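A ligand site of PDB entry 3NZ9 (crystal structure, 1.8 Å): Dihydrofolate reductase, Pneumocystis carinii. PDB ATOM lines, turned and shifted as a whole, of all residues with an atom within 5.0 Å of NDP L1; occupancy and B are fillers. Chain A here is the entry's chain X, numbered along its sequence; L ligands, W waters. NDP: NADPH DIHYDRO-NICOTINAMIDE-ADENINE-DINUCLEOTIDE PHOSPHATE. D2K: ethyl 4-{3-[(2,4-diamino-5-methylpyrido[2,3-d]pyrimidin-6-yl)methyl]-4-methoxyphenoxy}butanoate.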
ATOM      1  N   ILE A  10      -5.821  38.063  -1.178  1.00  0.00           N
ATOM      2  CA  ILE A  10      -6.896  38.172  -0.180  1.00  0.00           C
ATOM      3  C   ILE A  10      -6.525  37.233   1.021  1.00  0.00           C
ATOM      4  O   ILE A  10      -6.098  36.067   0.834  1.00  0.00           O
ATOM      5  CB  ILE A  10      -8.336  37.847  -0.734  1.00  0.00           C
ATOM      6  CG1 ILE A  10      -9.399  38.060   0.385  1.00  0.00           C
ATOM      7  CG2 ILE A  10      -8.396  36.448  -1.386  1.00  0.00           C
ATOM      8  CD1 ILE A  10     -10.908  38.238  -0.147  1.00  0.00           C
ATOM      9  N   VAL A  11      -6.663  37.783   2.205  1.00  0.00           N
ATOM     10  CA  VAL A  11      -6.101  37.192   3.444  1.00  0.00           C
ATOM     11  C   VAL A  11      -6.879  37.718   4.660  1.00  0.00           C
ATOM     12  O   VAL A  11      -7.379  38.853   4.709  1.00  0.00           O
ATOM     13  CB  VAL A  11      -4.535  37.521   3.609  1.00  0.00           C
ATOM     14  CG1 VAL A  11      -4.271  39.009   3.831  1.00  0.00           C
ATOM     15  CG2 VAL A  11      -3.916  36.695   4.754  1.00  0.00           C
ATOM     16  N   ALA A  12      -6.984  36.846   5.680  1.00  0.00           N
ATOM     17  CA  ALA A  12      -7.492  37.186   7.030  1.00  0.00           C
ATOM     18  C   ALA A  12      -6.292  36.974   7.928  1.00  0.00           C
ATOM     19  O   ALA A  12      -5.595  35.895   7.838  1.00  0.00           O
ATOM     20  CB  ALA A  12      -8.598  36.254   7.420  1.00  0.00           C
ATOM     21  N   LEU A  13      -5.966  37.989   8.714  1.00  0.00           N
ATOM     22  CA  LEU A  13      -4.742  37.918   9.514  1.00  0.00           C
ATOM     23  C   LEU A  13      -4.843  38.618  10.855  1.00  0.00           C
ATOM     24  O   LEU A  13      -5.607  39.589  11.007  1.00  0.00           O
ATOM     25  CB  LEU A  13      -3.476  38.391   8.748  1.00  0.00           C
ATOM     26  CG  LEU A  13      -3.211  39.882   8.636  1.00  0.00           C
ATOM     27  CD1 LEU A  13      -1.899  40.034   7.892  1.00  0.00           C
ATOM     28  CD2 LEU A  13      -4.262  40.493   7.761  1.00  0.00           C
ATOM     29  N   ILE A  19      -1.730  33.840  10.261  1.00  0.00           N
ATOM     30  CA  ILE A  19      -2.756  33.386   9.299  1.00  0.00           C
ATOM     31  C   ILE A  19      -3.197  31.952   9.460  1.00  0.00           C
ATOM     32  O   ILE A  19      -4.195  31.567   8.913  1.00  0.00           O
ATOM     33  CB  ILE A  19      -2.342  33.582   7.812  1.00  0.00           C
ATOM     34  CG1 ILE A  19      -1.059  32.805   7.465  1.00  0.00           C
ATOM     35  CG2 ILE A  19      -2.076  35.153   7.577  1.00  0.00           C
ATOM     36  CD1 ILE A  19      -0.670  32.820   5.952  1.00  0.00           C
ATOM     37  N   GLY A  20      -2.507  31.149  10.259  1.00  0.00           N
ATOM     38  CA  GLY A  20      -2.982  29.763  10.248  1.00  0.00           C
ATOM     39  C   GLY A  20      -2.400  28.993  11.415  1.00  0.00           C
ATOM     40  O   GLY A  20      -1.549  29.464  12.101  1.00  0.00           O
ATOM     41  N   ARG A  21      -2.896  27.772  11.596  1.00  0.00           N
ATOM     42  CA  ARG A  21      -2.462  26.918  12.691  1.00  0.00           C
ATOM     43  C   ARG A  21      -2.964  25.497  12.381  1.00  0.00           C
ATOM     44  O   ARG A  21      -4.154  25.288  12.020  1.00  0.00           O
ATOM     45  CB  ARG A  21      -3.060  27.389  14.016  1.00  0.00           C
ATOM     46  CG  ARG A  21      -2.712  26.476  15.171  1.00  0.00           C
ATOM     47  CD  ARG A  21      -1.973  27.133  16.265  1.00  0.00           C
ATOM     48  NE  ARG A  21      -1.148  26.173  17.027  1.00  0.00           N
ATOM     49  CZ  ARG A  21      -1.553  25.543  18.133  1.00  0.00           C
ATOM     50  NH1 ARG A  21      -2.783  25.727  18.616  1.00  0.00           N
ATOM     51  NH2 ARG A  21      -0.719  24.728  18.755  1.00  0.00           N
ATOM     52  N   ASN A  23      -2.386  23.381   9.869  1.00  0.00           N
ATOM     53  CA  ASN A  23      -2.945  23.476   8.515  1.00  0.00           C
ATOM     54  C   ASN A  23      -4.437  23.831   8.386  1.00  0.00           C
ATOM     55  O   ASN A  23      -5.145  23.314   7.513  1.00  0.00           O
ATOM     56  CB  ASN A  23      -2.638  22.225   7.671  1.00  0.00           C
ATOM     57  CG  ASN A  23      -2.298  22.570   6.222  1.00  0.00           C
ATOM     58  OD1 ASN A  23      -2.991  22.128   5.282  1.00  0.00           O
ATOM     59  ND2 ASN A  23      -1.258  23.382   6.035  1.00  0.00           N
ATOM     60  N   SER A  24      -4.919  24.730   9.249  1.00  0.00           N
ATOM     61  CA  SER A  24      -6.287  25.274   9.116  1.00  0.00           C
ATOM     62  C   SER A  24      -6.318  26.734   9.632  1.00  0.00           C
ATOM     63  O   SER A  24      -5.286  27.283   9.967  1.00  0.00           O
ATOM     64  CB  SER A  24      -7.308  24.420   9.882  1.00  0.00           C
ATOM     65  OG  SER A  24      -7.282  24.746  11.256  1.00  0.00           O
ATOM     66  N   LEU A  25      -7.488  27.345   9.686  1.00  0.00           N
ATOM     67  CA  LEU A  25      -7.643  28.673  10.302  1.00  0.00           C
ATOM     68  C   LEU A  25      -7.906  28.573  11.784  1.00  0.00           C
ATOM     69  O   LEU A  25      -8.846  27.870  12.184  1.00  0.00           O
ATOM     70  CB  LEU A  25      -8.813  29.441   9.649  1.00  0.00           C
ATOM     71  CG  LEU A  25      -8.574  29.487   8.137  1.00  0.00           C
ATOM     72  CD1 LEU A  25      -9.792  30.033   7.429  1.00  0.00           C
ATOM     73  CD2 LEU A  25      -7.357  30.372   7.883  1.00  0.00           C
ATOM     74  N   TRP A  27      -9.568  30.354  13.568  1.00  0.00           N
ATOM     75  CA  TRP A  27     -10.795  31.004  13.993  1.00  0.00           C
ATOM     76  C   TRP A  27     -11.892  30.358  13.165  1.00  0.00           C
ATOM     77  O   TRP A  27     -11.630  29.679  12.160  1.00  0.00           O
ATOM     78  CB  TRP A  27     -10.735  32.539  13.823  1.00  0.00           C
ATOM     79  CG  TRP A  27     -10.171  32.918  12.521  1.00  0.00           C
ATOM     80  CD1 TRP A  27     -10.792  32.807  11.300  1.00  0.00           C
ATOM     81  CD2 TRP A  27      -8.811  33.324  12.269  1.00  0.00           C
ATOM     82  NE1 TRP A  27      -9.889  33.205  10.304  1.00  0.00           N
ATOM     83  CE2 TRP A  27      -8.689  33.506  10.877  1.00  0.00           C
ATOM     84  CE3 TRP A  27      -7.701  33.574  13.080  1.00  0.00           C
ATOM     85  CZ2 TRP A  27      -7.501  33.941  10.272  1.00  0.00           C
ATOM     86  CZ3 TRP A  27      -6.502  34.009  12.475  1.00  0.00           C
ATOM     87  CH2 TRP A  27      -6.421  34.205  11.087  1.00  0.00           C
ATOM     88  N   GLY A  58      -1.775  27.715  -2.810  1.00  0.00           N
ATOM     89  CA  GLY A  58      -0.770  26.678  -2.611  1.00  0.00           C
ATOM     90  C   GLY A  58      -1.430  25.311  -2.327  1.00  0.00           C
ATOM     91  O   GLY A  58      -2.624  25.199  -2.068  1.00  0.00           O
ATOM     92  N   ARG A  59      -0.613  24.265  -2.432  1.00  0.00           N
ATOM     93  CA  ARG A  59      -1.111  22.931  -2.259  1.00  0.00           C
ATOM     94  C   ARG A  59      -1.549  22.744  -0.805  1.00  0.00           C
ATOM     95  O   ARG A  59      -2.534  22.084  -0.583  1.00  0.00           O
ATOM     96  CB  ARG A  59       0.015  21.939  -2.629  1.00  0.00           C
ATOM     97  CG  ARG A  59      -0.508  20.548  -2.950  1.00  0.00           C
ATOM     98  CD  ARG A  59      -0.032  19.549  -1.919  1.00  0.00           C
ATOM     99  NE  ARG A  59       1.378  19.726  -1.566  1.00  0.00           N
ATOM    100  CZ  ARG A  59       1.880  19.438  -0.371  1.00  0.00           C
ATOM    101  NH1 ARG A  59       3.162  19.645  -0.097  1.00  0.00           N
ATOM    102  NH2 ARG A  59       1.081  18.956   0.567  1.00  0.00           N
ATOM    103  N   LYS A  60      -0.831  23.296   0.170  1.00  0.00           N
ATOM    104  CA  LYS A  60      -1.251  23.111   1.595  1.00  0.00           C
ATOM    105  C   LYS A  60      -2.576  23.820   1.926  1.00  0.00           C
ATOM    106  O   LYS A  60      -3.390  23.300   2.698  1.00  0.00           O
ATOM    107  CB  LYS A  60      -0.134  23.441   2.590  1.00  0.00           C
ATOM    108  CG  LYS A  60       1.132  22.631   2.406  1.00  0.00           C
ATOM    109  CD  LYS A  60       2.266  23.186   3.216  1.00  0.00           C
ATOM    110  CE  LYS A  60       3.570  22.812   2.585  1.00  0.00           C
ATOM    111  NZ  LYS A  60       4.718  23.090   3.487  1.00  0.00           N
ATOM    112  N   THR A  61      -2.854  24.977   1.295  1.00  0.00           N
ATOM    113  CA  THR A  61      -4.213  25.591   1.366  1.00  0.00           C
ATOM    114  C   THR A  61      -5.319  24.778   0.697  1.00  0.00           C
ATOM    115  O   THR A  61      -6.504  24.700   1.164  1.00  0.00           O
ATOM    116  CB  THR A  61      -4.133  27.073   0.749  1.00  0.00           C
ATOM    117  OG1 THR A  61      -3.209  27.805   1.534  1.00  0.00           O
ATOM    118  CG2 THR A  61      -5.460  27.750   0.722  1.00  0.00           C
ATOM    119  N   SER A  64      -6.068  22.144   3.059  1.00  0.00           N
ATOM    120  CA  SER A  64      -6.656  22.817   4.234  1.00  0.00           C
ATOM    121  C   SER A  64      -8.137  23.014   4.136  1.00  0.00           C
ATOM    122  O   SER A  64      -8.823  23.000   5.133  1.00  0.00           O
ATOM    123  CB  SER A  64      -6.044  24.214   4.434  1.00  0.00           C
ATOM    124  OG  SER A  64      -6.648  24.886   5.546  1.00  0.00           O
ATOM    125  N   ILE A  80      -0.998  25.661  -7.057  1.00  0.00           N
ATOM    126  CA  ILE A  80       0.418  25.861  -7.322  1.00  0.00           C
ATOM    127  C   ILE A  80       1.234  24.808  -6.531  1.00  0.00           C
ATOM    128  O   ILE A  80       1.181  24.770  -5.298  1.00  0.00           O
ATOM    129  CB  ILE A  80       0.864  27.214  -6.841  1.00  0.00           C
ATOM    130  CG1 ILE A  80      -0.048  28.321  -7.364  1.00  0.00           C
ATOM    131  CG2 ILE A  80       2.371  27.426  -7.206  1.00  0.00           C
ATOM    132  CD1 ILE A  80      -0.473  28.204  -8.866  1.00  0.00           C
ATOM    133  N   THR A  81       1.982  23.947  -7.228  1.00  0.00           N
ATOM    134  CA  THR A  81       2.872  22.990  -6.515  1.00  0.00           C
ATOM    135  C   THR A  81       4.173  22.699  -7.311  1.00  0.00           C
ATOM    136  O   THR A  81       4.220  22.826  -8.516  1.00  0.00           O
ATOM    137  CB  THR A  81       2.094  21.666  -6.097  1.00  0.00           C
ATOM    138  OG1 THR A  81       3.020  20.579  -5.873  1.00  0.00           O
ATOM    139  CG2 THR A  81       1.059  21.206  -7.172  1.00  0.00           C
ATOM    140  N   ARG A  82       5.252  22.349  -6.627  1.00  0.00           N
ATOM    141  CA  ARG A  82       6.532  22.150  -7.329  1.00  0.00           C
ATOM    142  C   ARG A  82       6.598  20.751  -7.914  1.00  0.00           C
ATOM    143  O   ARG A  82       7.685  20.283  -8.257  1.00  0.00           O
ATOM    144  CB  ARG A  82       7.675  22.367  -6.359  1.00  0.00           C
ATOM    145  CG  ARG A  82       8.847  22.936  -6.945  1.00  0.00           C
ATOM    146  CD  ARG A  82       8.793  24.410  -6.918  1.00  0.00           C
ATOM    147  NE  ARG A  82       9.099  24.976  -5.607  1.00  0.00           N
ATOM    148  CZ  ARG A  82       9.366  26.269  -5.429  1.00  0.00           C
ATOM    149  NH1 ARG A  82       9.406  27.074  -6.490  1.00  0.00           N
ATOM    150  NH2 ARG A  82       9.631  26.744  -4.221  1.00  0.00           N
ATOM    151  N   LYS A  96       3.384  25.086 -11.586  1.00  0.00           N
ATOM    152  CA  LYS A  96       4.504  24.947 -10.690  1.00  0.00           C
ATOM    153  C   LYS A  96       4.961  26.270 -10.198  1.00  0.00           C
ATOM    154  O   LYS A  96       5.948  26.368  -9.494  1.00  0.00           O
ATOM    155  CB  LYS A  96       5.693  24.155 -11.293  1.00  0.00           C
ATOM    156  CG  LYS A  96       6.148  24.600 -12.602  1.00  0.00           C
ATOM    157  CD  LYS A  96       7.207  23.573 -13.147  1.00  0.00           C
ATOM    158  CE  LYS A  96       7.064  23.507 -14.655  1.00  0.00           C
ATOM    159  NZ  LYS A  96       8.388  23.491 -15.348  1.00  0.00           N
ATOM    160  N   SER A  97       4.257  27.324 -10.629  1.00  0.00           N
ATOM    161  CA  SER A  97       4.610  28.630 -10.165  1.00  0.00           C
ATOM    162  C   SER A  97       3.494  29.613 -10.480  1.00  0.00           C
ATOM    163  O   SER A  97       2.548  29.321 -11.245  1.00  0.00           O
ATOM    164  CB  SER A  97       5.922  29.146 -10.761  1.00  0.00           C
ATOM    165  OG  SER A  97       5.676  29.670 -12.053  1.00  0.00           O
ATOM    166  N   ILE A 123      -4.962  33.350  -2.873  1.00  0.00           N
ATOM    167  CA  ILE A 123      -5.753  33.211  -1.676  1.00  0.00           C
ATOM    168  C   ILE A 123      -5.016  32.464  -0.585  1.00  0.00           C
ATOM    169  O   ILE A 123      -5.633  32.170   0.450  1.00  0.00           O
ATOM    170  CB  ILE A 123      -7.065  32.410  -1.949  1.00  0.00           C
ATOM    171  CG1 ILE A 123      -6.780  30.985  -2.441  1.00  0.00           C
ATOM    172  CG2 ILE A 123      -7.880  33.092  -3.002  1.00  0.00           C
ATOM    173  CD1 ILE A 123      -7.976  29.992  -2.161  1.00  0.00           C
ATOM    174  N   GLY A 124      -3.735  32.203  -0.808  1.00  0.00           N
ATOM    175  CA  GLY A 124      -2.868  31.619   0.248  1.00  0.00           C
ATOM    176  C   GLY A 124      -2.145  30.365  -0.199  1.00  0.00           C
ATOM    177  O   GLY A 124      -2.352  29.933  -1.330  1.00  0.00           O
ATOM    178  N   GLY A 125      -1.268  29.775   0.635  1.00  0.00           N
ATOM    179  CA  GLY A 125      -0.962  30.276   1.962  1.00  0.00           C
ATOM    180  C   GLY A 125       0.299  31.046   2.001  1.00  0.00           C
ATOM    181  O   GLY A 125       0.608  31.745   1.058  1.00  0.00           O
ATOM    182  N   ALA A 126       1.057  30.943   3.102  1.00  0.00           N
ATOM    183  CA  ALA A 126       2.167  31.865   3.344  1.00  0.00           C
ATOM    184  C   ALA A 126       3.170  31.746   2.216  1.00  0.00           C
ATOM    185  O   ALA A 126       3.782  32.755   1.796  1.00  0.00           O
ATOM    186  CB  ALA A 126       2.874  31.604   4.694  1.00  0.00           C
ATOM    187  N   GLN A 127       3.431  30.540   1.749  1.00  0.00           N
ATOM    188  CA  GLN A 127       4.505  30.446   0.738  1.00  0.00           C
ATOM    189  C   GLN A 127       4.086  31.091  -0.601  1.00  0.00           C
ATOM    190  O   GLN A 127       4.885  31.828  -1.243  1.00  0.00           O
ATOM    191  CB  GLN A 127       4.879  29.003   0.571  1.00  0.00           C
ATOM    192  CG  GLN A 127       5.823  28.555   1.687  1.00  0.00           C
ATOM    193  CD  GLN A 127       6.293  27.155   1.472  1.00  0.00           C
ATOM    194  OE1 GLN A 127       6.437  26.709   0.331  1.00  0.00           O
ATOM    195  NE2 GLN A 127       6.489  26.427   2.576  1.00  0.00           N
ATOM    196  N   LEU A 128       2.824  30.856  -0.986  1.00  0.00           N
ATOM    197  CA  LEU A 128       2.315  31.515  -2.210  1.00  0.00           C
ATOM    198  C   LEU A 128       2.115  33.024  -2.025  1.00  0.00           C
ATOM    199  O   LEU A 128       2.332  33.763  -3.007  1.00  0.00           O
ATOM    200  CB  LEU A 128       0.985  30.879  -2.718  1.00  0.00           C
ATOM    201  CG  LEU A 128       0.543  30.775  -4.189  1.00  0.00           C
ATOM    202  CD1 LEU A 128      -0.927  30.951  -4.603  1.00  0.00           C
ATOM    203  CD2 LEU A 128       1.579  31.190  -5.266  1.00  0.00           C
ATOM    204  N   TYR A 129       1.747  33.477  -0.813  1.00  0.00           N
ATOM    205  CA  TYR A 129       1.674  34.905  -0.531  1.00  0.00           C
ATOM    206  C   TYR A 129       3.048  35.529  -0.669  1.00  0.00           C
ATOM    207  O   TYR A 129       3.171  36.627  -1.182  1.00  0.00           O
ATOM    208  CB  TYR A 129       1.212  35.168   0.895  1.00  0.00           C
ATOM    209  CG  TYR A 129      -0.285  34.935   1.157  1.00  0.00           C
ATOM    210  CD1 TYR A 129      -1.264  35.328   0.225  1.00  0.00           C
ATOM    211  CD2 TYR A 129      -0.706  34.452   2.389  1.00  0.00           C
ATOM    212  CE1 TYR A 129      -2.628  35.177   0.496  1.00  0.00           C
ATOM    213  CE2 TYR A 129      -2.068  34.334   2.684  1.00  0.00           C
ATOM    214  CZ  TYR A 129      -3.009  34.678   1.738  1.00  0.00           C
ATOM    215  OH  TYR A 129      -4.347  34.549   2.079  1.00  0.00           O
ATOM    216  N   ALA A 131       5.464  34.563  -2.693  1.00  0.00           N
ATOM    217  CA  ALA A 131       5.700  34.698  -4.148  1.00  0.00           C
ATOM    218  C   ALA A 131       4.898  35.853  -4.684  1.00  0.00           C
ATOM    219  O   ALA A 131       5.357  36.607  -5.544  1.00  0.00           O
ATOM    220  CB  ALA A 131       5.324  33.469  -4.889  1.00  0.00           C
ATOM    221  N   VAL A 154       1.743  29.741  11.352  1.00  0.00           N
ATOM    222  CA  VAL A 154       2.137  30.216  10.036  1.00  0.00           C
ATOM    223  C   VAL A 154       1.768  31.702   9.900  1.00  0.00           C
ATOM    224  O   VAL A 154       0.709  32.113  10.342  1.00  0.00           O
ATOM    225  CB  VAL A 154       1.435  29.411   8.935  1.00  0.00           C
ATOM    226  CG1 VAL A 154       1.527  30.087   7.582  1.00  0.00           C
ATOM    227  CG2 VAL A 154       2.039  27.948   8.775  1.00  0.00           C
HETATM  228  PA  NDP L   1       0.713  27.092   1.048  1.00  0.00           P
HETATM  229  O1A NDP L   1      -0.728  26.851   0.807  1.00  0.00           O
HETATM  230  O2A NDP L   1       1.421  28.290   0.427  1.00  0.00           O
HETATM  231  O5B NDP L   1       1.374  25.787   0.240  1.00  0.00           O
HETATM  232  C5B NDP L   1       2.761  25.674   0.396  1.00  0.00           C
HETATM  233  C4B NDP L   1       3.055  24.714  -0.647  1.00  0.00           C
HETATM  234  O4B NDP L   1       2.269  25.141  -1.906  1.00  0.00           O
HETATM  235  C3B NDP L   1       4.476  24.425  -1.112  1.00  0.00           C
HETATM  236  O3B NDP L   1       5.102  23.502  -0.216  1.00  0.00           O
HETATM  237  C2B NDP L   1       3.744  23.705  -2.218  1.00  0.00           C
HETATM  238  O2B NDP L   1       4.397  23.016  -3.109  1.00  0.00           O
HETATM  239  C1B NDP L   1       3.167  24.948  -2.959  1.00  0.00           C
HETATM  240  N9A NDP L   1       3.832  26.383  -3.303  1.00  0.00           N
HETATM  241  C8A NDP L   1       3.618  27.560  -2.643  1.00  0.00           C
HETATM  242  N7A NDP L   1       4.279  28.592  -3.193  1.00  0.00           N
HETATM  243  C5A NDP L   1       4.898  28.096  -4.287  1.00  0.00           C
HETATM  244  C6A NDP L   1       5.723  28.645  -5.286  1.00  0.00           C
HETATM  245  N6A NDP L   1       6.083  29.951  -5.314  1.00  0.00           N
HETATM  246  N1A NDP L   1       6.185  27.826  -6.269  1.00  0.00           N
HETATM  247  C2A NDP L   1       5.880  26.523  -6.303  1.00  0.00           C
HETATM  248  N3A NDP L   1       5.109  25.957  -5.374  1.00  0.00           N
HETATM  249  C4A NDP L   1       4.608  26.710  -4.357  1.00  0.00           C
HETATM  250  O3  NDP L   1       1.159  26.677   2.545  1.00  0.00           O
HETATM  251  PN  NDP L   1       1.687  27.523   3.828  1.00  0.00           P
HETATM  252  O1N NDP L   1       2.743  28.519   3.546  1.00  0.00           O
HETATM  253  O2N NDP L   1       2.031  26.357   4.751  1.00  0.00           O
HETATM  254  O5D NDP L   1       0.353  28.229   4.387  1.00  0.00           O
HETATM  255  C5D NDP L   1      -0.766  27.401   4.715  1.00  0.00           C
HETATM  256  C4D NDP L   1      -1.374  27.793   6.071  1.00  0.00           C
HETATM  257  O4D NDP L   1      -2.013  29.043   5.649  1.00  0.00           O
HETATM  258  C3D NDP L   1      -2.498  26.888   6.585  1.00  0.00           C
HETATM  259  O3D NDP L   1      -2.629  27.056   8.033  1.00  0.00           O
HETATM  260  C2D NDP L   1      -3.727  27.520   5.963  1.00  0.00           C
HETATM  261  O2D NDP L   1      -4.873  27.253   6.790  1.00  0.00           O
HETATM  262  C1D NDP L   1      -3.348  28.997   6.117  1.00  0.00           C
HETATM  263  N1N NDP L   1      -4.119  29.953   5.286  1.00  0.00           N
HETATM  264  C2N NDP L   1      -4.597  31.132   5.906  1.00  0.00           C
HETATM  265  C3N NDP L   1      -5.314  32.013   5.122  1.00  0.00           C
HETATM  266  C7N NDP L   1      -5.912  33.293   5.745  1.00  0.00           C
HETATM  267  O7N NDP L   1      -6.478  34.084   4.984  1.00  0.00           O
HETATM  268  N7N NDP L   1      -5.891  33.315   7.118  1.00  0.00           N
HETATM  269  C4N NDP L   1      -5.531  31.769   3.735  1.00  0.00           C
HETATM  270  C5N NDP L   1      -5.072  30.612   3.112  1.00  0.00           C
HETATM  271  C6N NDP L   1      -4.336  29.711   3.886  1.00  0.00           C
HETATM  272  P2B NDP L   1       5.078  21.545  -2.977  1.00  0.00           P
HETATM  273  O1X NDP L   1       3.815  20.695  -3.478  1.00  0.00           O
HETATM  274  O2X NDP L   1       5.363  21.256  -1.401  1.00  0.00           O
HETATM  275  O3X NDP L   1       6.280  21.836  -3.857  1.00  0.00           O
HETATM  276  N1  D2K L   2      -8.977  35.244   2.838  1.00  0.00           N
HETATM  277  C2  D2K L   2      -9.907  35.612   3.729  1.00  0.00           C
HETATM  278  N3  D2K L   2     -10.642  34.671   4.328  1.00  0.00           N
HETATM  279  C4  D2K L   2     -10.481  33.372   4.005  1.00  0.00           C
HETATM  280  C5  D2K L   2      -9.551  32.968   3.012  1.00  0.00           C
HETATM  281  C6  D2K L   2      -8.743  33.992   2.427  1.00  0.00           C
HETATM  282  CAA D2K L   2     -20.124  27.560   1.945  1.00  0.00           C
HETATM  283  CAB D2K L   2      -7.702  27.984   3.602  1.00  0.00           C
HETATM  284  CAC D2K L   2      -8.567  30.957   1.669  1.00  0.00           C
HETATM  285  NAD D2K L   2     -10.076  36.931   4.076  1.00  0.00           N
HETATM  286  NAE D2K L   2      -7.771  33.800   1.524  1.00  0.00           N
HETATM  287  OAF D2K L   2     -16.288  27.758   0.545  1.00  0.00           O
HETATM  288  CAG D2K L   2     -11.554  26.540   5.966  1.00  0.00           C
HETATM  289  CAH D2K L   2     -10.189  26.841   5.898  1.00  0.00           C
HETATM  290  CAI D2K L   2     -11.210  31.187   4.342  1.00  0.00           C
HETATM  291  CAJ D2K L   2     -11.994  28.023   4.113  1.00  0.00           C
HETATM  292  CAK D2K L   2     -18.903  28.138   2.700  1.00  0.00           C
HETATM  293  CAL D2K L   2     -15.525  26.946   3.430  1.00  0.00           C
HETATM  294  CAM D2K L   2     -14.087  26.621   3.750  1.00  0.00           C
HETATM  295  CAN D2K L   2     -15.623  28.301   2.755  1.00  0.00           C
HETATM  296  CAO D2K L   2     -10.236  29.256   2.984  1.00  0.00           C
HETATM  297  NAP D2K L   2     -11.272  32.492   4.650  1.00  0.00           N
HETATM  298  OAS D2K L   2      -8.344  28.015   4.863  1.00  0.00           O
HETATM  299  OAT D2K L   2     -17.942  28.751   1.765  1.00  0.00           O
HETATM  300  OAU D2K L   2     -13.768  26.825   5.161  1.00  0.00           O
HETATM  301  CAV D2K L   2     -16.658  28.228   1.622  1.00  0.00           C
HETATM  302  CAX D2K L   2     -12.445  27.119   5.089  1.00  0.00           C
HETATM  303  CAZ D2K L   2      -9.501  31.608   2.687  1.00  0.00           C
HETATM  304  CBA D2K L   2     -10.329  30.733   3.371  1.00  0.00           C
HETATM  305  CBB D2K L   2     -10.638  28.315   4.067  1.00  0.00           C
HETATM  306  CBC D2K L   2      -9.709  27.716   4.917  1.00  0.00           C
HETATM  307  O   HOH W   1       4.658  25.614   4.397  1.00  0.00           O
HETATM  308  O   HOH W   2       1.174  25.058   7.121  1.00  0.00           O
HETATM  309  O   HOH W   3       5.016  28.566   4.946  1.00  0.00           O
HETATM  310  O   HOH W   4       5.495  31.347  -7.793  1.00  0.00           O
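Water W1 lies within hydrogen-bond range of the side-chain amino group (NZ) of Lys 60, the side-chain amide nitrogen (NE2) of Gln 127 and an oxygen (O2N) of NDP L1. Water W2 bridges an oxygen (O2N) of NDP L1 and the side-chain amide nitrogen (ND2) of Asn 23.
O of Ile 80 lies within hydrogen-bond range of N of Arg 59. The backbone carbonyl oxygen of Val 154 sits at hydrogen-bond distance from the backbone NH of Ile 19, 3.0 Å away. The side-chain hydroxyl of Ser 24 is in hydrogen-bond range of the backbone carbonyl oxygen of Arg 21 (3.3 Å). The backbone carbonyl oxygen (O) of Asn 23 is in hydrogen-bond range of the side-chain hydroxyl (OG) of Ser 64 (2.9 Å). O of Lys 60 sits close to OD1 of Asn 23. O of Gly 124 is in hydrogen-bond range of N of Gly 58, 2.7 Å away. The side-chain hydroxyl (OH) of Tyr 129 is in hydrogen-bond range of the backbone carbonyl oxygen (O) of Ile 10 (2.6 Å). The backbone NH (N) of Gly 20 lies within hydrogen-bond range of the backbone carbonyl oxygen (O) of Val 154 (3.4 Å).
OG1 of Thr 81 lies within hydrogen-bond range of O1X of NDP L1 (2.5 Å). The backbone NH of Ala 12 is in hydrogen-bond range of an oxygen (O7N) of NDP L1 (2.9 Å). N7N of NDP L1 is in hydrogen-bond range of O of Ala 12, 2.7 Å away. The backbone NH of Thr 61 sits at hydrogen-bond distance from an oxygen (O1A) of NDP L1. An oxygen (O1A) of NDP L1 is in hydrogen-bond range of the side-chain hydroxyl (OG1) of Thr 61, at 2.8 Å. O1N of NDP L1 sits at hydrogen-bond distance from N of Gln 127, at 2.8 Å. An oxygen (O3X) of NDP L1 sits close to the backbone NH (N) of Arg 82 (3.0 Å). The guanidinium group (NH1) of Arg 82 sits at hydrogen-bond distance from a nitrogen (N1A) of NDP L1. The backbone NH of Gly 125 sits at hydrogen-bond distance from an oxygen (O1A) of NDP L1, at 3.0 Å. O1N of NDP L1 lies within hydrogen-bond range of N of Ala 126 (3.0 Å). The backbone NH (N) of Arg 59 is in hydrogen-bond range of an oxygen (O4B) of NDP L1. O2X of NDP L1 is in salt-bridge range of NH1 of Arg 59 (3.0 Å). O of Ile 19 sits at hydrogen-bond distance from N7N of NDP L1, at 3.0 Å. The backbone NH (N) of Ser 24 is in hydrogen-bond range of an oxygen (O3D) of NDP L1, at 3.5 Å. The backbone carbonyl oxygen of Ser 24 lies within hydrogen-bond range of an oxygen (O2D) of NDP L1 (3.2 Å). An oxygen (O2D) of NDP L1 lies within hydrogen-bond range of the side-chain hydroxyl of Ser 64 (3.2 Å). An oxygen (O2A) of NDP L1 lies within hydrogen-bond range of the backbone NH of Leu 128. N of Lys 60 lies within hydrogen-bond range of O5B of NDP L1. The backbone carbonyl oxygen (O) of Ile 123 lies within hydrogen-bond range of a nitrogen (NAE) of D2K L2 (2.9 Å). A nitrogen (N1) of D2K L2 lies within hydrogen-bond range of the backbone NH (N) of Val 11 (3.5 Å). O of Val 11 sits close to NAD of D2K L2 (3.4 Å). A nitrogen (NAE) of D2K L2 sits at hydrogen-bond distance from the backbone carbonyl oxygen (O) of Ile 10.
Residues that only touch NDP L1: Val 11 (3.5 Å), Gly 20 (3.5 Å), Arg 21 (3.6 Å), Asn 23 (3.6 Å), Leu 25 (3.4 Å), Trp 27 (3.6 Å), Gly 58 (3.4 Å), Ile 80 (3.1 Å), Lys 96 (3.2 Å), Ile 123 (3.1 Å), Gly 124 (3.8 Å), Tyr 129 (3.4 Å), Ala 131 (3.6 Å) and Val 154 (3.9 Å). Within 4 Å of NDP L1: Val 11, Ala 12, Ile 19, Gly 20, Arg 21, Asn 23, Ser 24, Leu 25, Trp 27, Gly 58, Arg 59, Lys 60, Thr 61, Ser 64, Ile 80, Thr 81, Arg 82, Lys 96, Ile 123, Gly 124, Gly 125, Ala 126, Gln 127, Leu 128, Tyr 129, Ala 131 and Val 154. The nearest printed residue that does not touch NDP L1 is Ser 97 (4.3 Å).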
